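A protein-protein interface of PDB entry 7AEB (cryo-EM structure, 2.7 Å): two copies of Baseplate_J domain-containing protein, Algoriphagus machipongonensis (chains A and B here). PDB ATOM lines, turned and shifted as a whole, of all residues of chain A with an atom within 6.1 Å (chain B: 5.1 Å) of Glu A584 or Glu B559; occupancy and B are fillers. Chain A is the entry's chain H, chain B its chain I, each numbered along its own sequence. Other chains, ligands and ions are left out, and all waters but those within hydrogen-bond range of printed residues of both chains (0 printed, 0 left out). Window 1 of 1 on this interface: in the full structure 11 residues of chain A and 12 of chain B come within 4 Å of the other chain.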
ATOM      1  N   HIS A 484       4.477   6.326  18.303  1.00  0.00           N
ATOM      2  CA  HIS A 484       4.656   6.849  16.954  1.00  0.00           C
ATOM      3  C   HIS A 484       3.439   7.607  16.441  1.00  0.00           C
ATOM      4  O   HIS A 484       3.591   8.569  15.685  1.00  0.00           O
ATOM      5  CB  HIS A 484       4.963   5.689  16.004  1.00  0.00           C
ATOM      6  CG  HIS A 484       5.415   6.111  14.643  1.00  0.00           C
ATOM      7  ND1 HIS A 484       6.703   6.517  14.386  1.00  0.00           N
ATOM      8  CD2 HIS A 484       4.755   6.182  13.464  1.00  0.00           C
ATOM      9  CE1 HIS A 484       6.819   6.825  13.107  1.00  0.00           C
ATOM     10  NE2 HIS A 484       5.650   6.632  12.526  1.00  0.00           N
ATOM     11  N   TYR A 485       2.232   7.204  16.849  1.00  0.00           N
ATOM     12  CA  TYR A 485       0.994   7.808  16.370  1.00  0.00           C
ATOM     13  C   TYR A 485       0.313   8.678  17.417  1.00  0.00           C
ATOM     14  O   TYR A 485      -0.898   8.891  17.331  1.00  0.00           O
ATOM     15  CB  TYR A 485       0.006   6.740  15.895  1.00  0.00           C
ATOM     16  CG  TYR A 485       0.469   5.960  14.710  1.00  0.00           C
ATOM     17  CD1 TYR A 485       0.305   6.435  13.421  1.00  0.00           C
ATOM     18  CD2 TYR A 485       1.066   4.746  14.887  1.00  0.00           C
ATOM     19  CE1 TYR A 485       0.743   5.706  12.343  1.00  0.00           C
ATOM     20  CE2 TYR A 485       1.507   4.013  13.834  1.00  0.00           C
ATOM     21  CZ  TYR A 485       1.347   4.493  12.560  1.00  0.00           C
ATOM     22  OH  TYR A 485       1.804   3.745  11.507  1.00  0.00           O
ATOM     23  N   TYR A 488      -2.123  11.547  16.348  1.00  0.00           N
ATOM     24  CA  TYR A 488      -3.313  11.206  15.582  1.00  0.00           C
ATOM     25  C   TYR A 488      -4.457  10.909  16.539  1.00  0.00           C
ATOM     26  O   TYR A 488      -4.632   9.772  16.973  1.00  0.00           O
ATOM     27  CB  TYR A 488      -3.067   9.988  14.725  1.00  0.00           C
ATOM     28  CG  TYR A 488      -2.050  10.097  13.639  1.00  0.00           C
ATOM     29  CD1 TYR A 488      -0.702  10.112  13.924  1.00  0.00           C
ATOM     30  CD2 TYR A 488      -2.438  10.105  12.317  1.00  0.00           C
ATOM     31  CE1 TYR A 488       0.223  10.170  12.938  1.00  0.00           C
ATOM     32  CE2 TYR A 488      -1.517  10.158  11.320  1.00  0.00           C
ATOM     33  CZ  TYR A 488      -0.187  10.191  11.637  1.00  0.00           C
ATOM     34  OH  TYR A 488       0.743  10.238  10.642  1.00  0.00           O
ATOM     35  N   TYR A 561      -2.523  11.462   7.157  1.00  0.00           N
ATOM     36  CA  TYR A 561      -1.334  12.246   7.477  1.00  0.00           C
ATOM     37  C   TYR A 561      -1.493  13.713   7.098  1.00  0.00           C
ATOM     38  O   TYR A 561      -1.234  14.599   7.916  1.00  0.00           O
ATOM     39  CB  TYR A 561      -0.126  11.661   6.776  1.00  0.00           C
ATOM     40  CG  TYR A 561       1.132  12.421   7.016  1.00  0.00           C
ATOM     41  CD1 TYR A 561       1.769  12.347   8.232  1.00  0.00           C
ATOM     42  CD2 TYR A 561       1.695  13.191   6.027  1.00  0.00           C
ATOM     43  CE1 TYR A 561       2.921  13.010   8.462  1.00  0.00           C
ATOM     44  CE2 TYR A 561       2.859  13.864   6.252  1.00  0.00           C
ATOM     45  CZ  TYR A 561       3.466  13.766   7.473  1.00  0.00           C
ATOM     46  OH  TYR A 561       4.632  14.438   7.712  1.00  0.00           O
ATOM     47  N   PRO A 582       2.705  15.235  13.288  1.00  0.00           N
ATOM     48  CA  PRO A 582       2.591  13.795  13.085  1.00  0.00           C
ATOM     49  C   PRO A 582       3.793  13.243  12.361  1.00  0.00           C
ATOM     50  O   PRO A 582       4.374  13.893  11.493  1.00  0.00           O
ATOM     51  CB  PRO A 582       1.332  13.672  12.226  1.00  0.00           C
ATOM     52  CG  PRO A 582       1.230  14.991  11.544  1.00  0.00           C
ATOM     53  CD  PRO A 582       1.728  15.992  12.504  1.00  0.00           C
ATOM     54  N   ASN A 583       4.145  12.024  12.717  1.00  0.00           N
ATOM     55  CA  ASN A 583       5.187  11.289  12.041  1.00  0.00           C
ATOM     56  C   ASN A 583       4.582  10.609  10.837  1.00  0.00           C
ATOM     57  O   ASN A 583       3.387  10.318  10.820  1.00  0.00           O
ATOM     58  CB  ASN A 583       5.776  10.243  12.961  1.00  0.00           C
ATOM     59  CG  ASN A 583       6.472  10.836  14.119  1.00  0.00           C
ATOM     60  OD1 ASN A 583       7.370  11.654  13.967  1.00  0.00           O
ATOM     61  ND2 ASN A 583       6.078  10.423  15.300  1.00  0.00           N
ATOM     62  N   GLU A 584       5.404  10.355   9.841  1.00  0.00           N
ATOM     63  CA  GLU A 584       4.942   9.626   8.669  1.00  0.00           C
ATOM     64  C   GLU A 584       4.465   8.242   9.085  1.00  0.00           C
ATOM     65  O   GLU A 584       5.127   7.580   9.896  1.00  0.00           O
ATOM     66  CB  GLU A 584       6.090   9.523   7.683  1.00  0.00           C
ATOM     67  CG  GLU A 584       6.440  10.864   7.130  1.00  0.00           C
ATOM     68  CD  GLU A 584       7.548  11.486   7.935  1.00  0.00           C
ATOM     69  OE1 GLU A 584       7.865  10.948   9.011  1.00  0.00           O
ATOM     70  OE2 GLU A 584       8.014  12.564   7.581  1.00  0.00           O
ATOM     71  N   PRO A 585       3.300   7.830   8.613  1.00  0.00           N
ATOM     72  CA  PRO A 585       2.743   6.503   8.869  1.00  0.00           C
ATOM     73  C   PRO A 585       3.673   5.397   8.412  1.00  0.00           C
ATOM     74  O   PRO A 585       4.361   5.522   7.399  1.00  0.00           O
ATOM     75  CB  PRO A 585       1.460   6.532   8.035  1.00  0.00           C
ATOM     76  CG  PRO A 585       1.120   7.976   7.963  1.00  0.00           C
ATOM     77  CD  PRO A 585       2.381   8.697   7.884  1.00  0.00           C
ATOM     78  N   TYR A 586       3.685   4.310   9.172  1.00  0.00           N
ATOM     79  CA  TYR A 586       4.564   3.178   8.912  1.00  0.00           C
ATOM     80  C   TYR A 586       4.025   2.248   7.826  1.00  0.00           C
ATOM     81  O   TYR A 586       2.827   1.963   7.758  1.00  0.00           O
ATOM     82  CB  TYR A 586       4.761   2.425  10.222  1.00  0.00           C
ATOM     83  CG  TYR A 586       5.618   1.201  10.184  1.00  0.00           C
ATOM     84  CD1 TYR A 586       6.955   1.278   9.878  1.00  0.00           C
ATOM     85  CD2 TYR A 586       5.087  -0.030  10.517  1.00  0.00           C
ATOM     86  CE1 TYR A 586       7.732   0.166   9.874  1.00  0.00           C
ATOM     87  CE2 TYR A 586       5.860  -1.144  10.525  1.00  0.00           C
ATOM     88  CZ  TYR A 586       7.180  -1.044  10.200  1.00  0.00           C
ATOM     89  OH  TYR A 586       7.964  -2.164  10.201  1.00  0.00           O
ATOM     90  N   ARG B 446      18.045   7.328  -1.215  1.00  0.00           N
ATOM     91  CA  ARG B 446      17.337   7.904  -0.078  1.00  0.00           C
ATOM     92  C   ARG B 446      17.430   6.917   1.082  1.00  0.00           C
ATOM     93  O   ARG B 446      16.458   6.225   1.399  1.00  0.00           O
ATOM     94  CB  ARG B 446      15.888   8.163  -0.473  1.00  0.00           C
ATOM     95  CG  ARG B 446      15.026   8.865   0.534  1.00  0.00           C
ATOM     96  CD  ARG B 446      13.662   9.044  -0.038  1.00  0.00           C
ATOM     97  NE  ARG B 446      12.726   9.604   0.928  1.00  0.00           N
ATOM     98  CZ  ARG B 446      12.515  10.903   1.130  1.00  0.00           C
ATOM     99  NH1 ARG B 446      13.180  11.820   0.442  1.00  0.00           N
ATOM    100  NH2 ARG B 446      11.624  11.285   2.034  1.00  0.00           N
ATOM    101  N   PRO B 447      18.602   6.816   1.717  1.00  0.00           N
ATOM    102  CA  PRO B 447      18.887   5.779   2.720  1.00  0.00           C
ATOM    103  C   PRO B 447      17.975   5.829   3.923  1.00  0.00           C
ATOM    104  O   PRO B 447      17.628   6.903   4.405  1.00  0.00           O
ATOM    105  CB  PRO B 447      20.311   6.119   3.158  1.00  0.00           C
ATOM    106  CG  PRO B 447      20.862   6.903   2.056  1.00  0.00           C
ATOM    107  CD  PRO B 447      19.752   7.693   1.506  1.00  0.00           C
ATOM    108  N   SER B 555      19.467   6.423   9.987  1.00  0.00           N
ATOM    109  CA  SER B 555      19.226   7.072   8.706  1.00  0.00           C
ATOM    110  C   SER B 555      19.928   8.419   8.609  1.00  0.00           C
ATOM    111  O   SER B 555      20.439   8.970   9.584  1.00  0.00           O
ATOM    112  CB  SER B 555      17.748   7.325   8.488  1.00  0.00           C
ATOM    113  OG  SER B 555      17.339   8.424   9.275  1.00  0.00           O
ATOM    114  N   LEU B 557      18.246  11.136   7.803  1.00  0.00           N
ATOM    115  CA  LEU B 557      17.193  12.111   8.124  1.00  0.00           C
ATOM    116  C   LEU B 557      16.460  12.680   6.912  1.00  0.00           C
ATOM    117  O   LEU B 557      15.985  13.812   6.977  1.00  0.00           O
ATOM    118  CB  LEU B 557      17.732  13.274   8.961  1.00  0.00           C
ATOM    119  CG  LEU B 557      18.496  12.922  10.228  1.00  0.00           C
ATOM    120  CD1 LEU B 557      19.090  14.177  10.816  1.00  0.00           C
ATOM    121  CD2 LEU B 557      17.556  12.269  11.207  1.00  0.00           C
ATOM    122  N   HIS B 558      16.305  11.912   5.833  1.00  0.00           N
ATOM    123  CA  HIS B 558      15.581  12.407   4.665  1.00  0.00           C
ATOM    124  C   HIS B 558      14.128  12.685   5.011  1.00  0.00           C
ATOM    125  O   HIS B 558      13.564  13.713   4.620  1.00  0.00           O
ATOM    126  CB  HIS B 558      15.711  11.395   3.529  1.00  0.00           C
ATOM    127  CG  HIS B 558      17.066  11.408   2.907  1.00  0.00           C
ATOM    128  ND1 HIS B 558      17.340  12.082   1.742  1.00  0.00           N
ATOM    129  CD2 HIS B 558      18.244  10.899   3.331  1.00  0.00           C
ATOM    130  CE1 HIS B 558      18.622  11.965   1.454  1.00  0.00           C
ATOM    131  NE2 HIS B 558      19.198  11.257   2.408  1.00  0.00           N
ATOM    132  N   GLU B 559      13.573  11.850   5.873  1.00  0.00           N
ATOM    133  CA  GLU B 559      12.203  11.912   6.352  1.00  0.00           C
ATOM    134  C   GLU B 559      11.894  13.127   7.228  1.00  0.00           C
ATOM    135  O   GLU B 559      10.722  13.350   7.541  1.00  0.00           O
ATOM    136  CB  GLU B 559      11.908  10.616   7.116  1.00  0.00           C
ATOM    137  CG  GLU B 559      12.751  10.378   8.379  1.00  0.00           C
ATOM    138  CD  GLU B 559      14.085   9.695   8.118  1.00  0.00           C
ATOM    139  OE1 GLU B 559      14.533   9.680   6.968  1.00  0.00           O
ATOM    140  OE2 GLU B 559      14.695   9.182   9.065  1.00  0.00           O
ATOM    141  N   LYS B 560      12.887  13.911   7.646  1.00  0.00           N
ATOM    142  CA  LYS B 560      12.626  15.062   8.495  1.00  0.00           C
ATOM    143  C   LYS B 560      12.793  16.403   7.814  1.00  0.00           C
ATOM    144  O   LYS B 560      12.486  17.413   8.448  1.00  0.00           O
ATOM    145  CB  LYS B 560      13.549  15.072   9.714  1.00  0.00           C
ATOM    146  CG  LYS B 560      13.418  13.906  10.637  1.00  0.00           C
ATOM    147  CD  LYS B 560      12.053  13.857  11.265  1.00  0.00           C
ATOM    148  CE  LYS B 560      11.980  12.787  12.320  1.00  0.00           C
ATOM    149  NZ  LYS B 560      10.621  12.705  12.922  1.00  0.00           N
ATOM    150  N   TYR B 561      13.293  16.446   6.582  1.00  0.00           N
ATOM    151  CA  TYR B 561      13.626  17.728   5.967  1.00  0.00           C
ATOM    152  C   TYR B 561      12.424  18.659   5.886  1.00  0.00           C
ATOM    153  O   TYR B 561      12.510  19.820   6.294  1.00  0.00           O
ATOM    154  CB  TYR B 561      14.200  17.503   4.585  1.00  0.00           C
ATOM    155  CG  TYR B 561      14.540  18.766   3.865  1.00  0.00           C
ATOM    156  CD1 TYR B 561      15.642  19.501   4.232  1.00  0.00           C
ATOM    157  CD2 TYR B 561      13.776  19.205   2.810  1.00  0.00           C
ATOM    158  CE1 TYR B 561      15.978  20.633   3.579  1.00  0.00           C
ATOM    159  CE2 TYR B 561      14.108  20.348   2.146  1.00  0.00           C
ATOM    160  CZ  TYR B 561      15.215  21.054   2.537  1.00  0.00           C
ATOM    161  OH  TYR B 561      15.559  22.201   1.880  1.00  0.00           O
ATOM    162  N   HIS B 563       9.666  18.793   7.630  1.00  0.00           N
ATOM    163  CA  HIS B 563       9.236  19.229   8.950  1.00  0.00           C
ATOM    164  C   HIS B 563      10.078  20.355   9.519  1.00  0.00           C
ATOM    165  O   HIS B 563       9.541  21.281  10.097  1.00  0.00           O
ATOM    166  CB  HIS B 563       9.297  18.064   9.917  1.00  0.00           C
ATOM    167  CG  HIS B 563       8.296  16.995   9.648  1.00  0.00           C
ATOM    168  ND1 HIS B 563       7.544  16.426  10.646  1.00  0.00           N
ATOM    169  CD2 HIS B 563       7.926  16.381   8.502  1.00  0.00           C
ATOM    170  CE1 HIS B 563       6.746  15.509  10.127  1.00  0.00           C
ATOM    171  NE2 HIS B 563       6.961  15.464   8.826  1.00  0.00           N
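Hydrophobic or aromatic side chains of chain B within 4 Å of the printed part of chain A: His B563.
Of the 9 printed residues of chain A, 4 touch a printed residue of chain B.
Hydrophobic or aromatic side chains of chain A within 4 Å of the printed part of chain B: Tyr A561.
Among the printed residues, 5 pairs touch across the chains.
Among the printed residues, no Asp or Glu carboxylate lies within 4 Å of a Lys or Arg side-chain nitrogen of the other chain.
The side-chain hydroxyl (OH) of Tyr A488 sits at hydrogen-bond distance from the backbone carbonyl oxygen (O) of Asn A583.
The backbone carbonyl oxygen of His A484 lies within hydrogen-bond range of the side-chain amide nitrogen of Asn A583, 3.1 Å away.
O of Glu A584 sits at hydrogen-bond distance from NE2 of His A484 (2.8 Å).
The side-chain hydroxyl (OG) of Ser B555 is in hydrogen-bond range of the side-chain carboxylate (OE2) of Glu B559 (2.8 Å).
Glu A584 touches two residues of chain B.
Glu B559 touches one residue of chain A.
Printed residues of chain B within 4 Å of Tyr A561: His B563.
Of the printed residues of chain A, Lys B560 touches Asn A583.
Printed residues of chain B within 4 Å of Pro A582: His B563 (3.2 Å).
Printed residues of chain B within 4 Å of Asn A583: Lys B560.
Arg B446 touches none of the printed residues of chain A.
Tyr A488 touches none of the printed residues of chain B.
The side-chain hydroxyl (OH) of Tyr A561 is in hydrogen-bond range of a ring nitrogen (NE2) of His B563 (2.8 Å).
The side-chain carboxylate (OE2) of Glu A584 sits at hydrogen-bond distance from a ring nitrogen (NE2) of His B563 (3.3 Å).
OE2 of Glu A584 sits close to O of Glu B559 (2.8 Å).
Position printed for both chains: 561.
Among the printed residues, pairs that only touch across the chains: Pro A582 with His B563 and Asn A583 with Lys B560.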
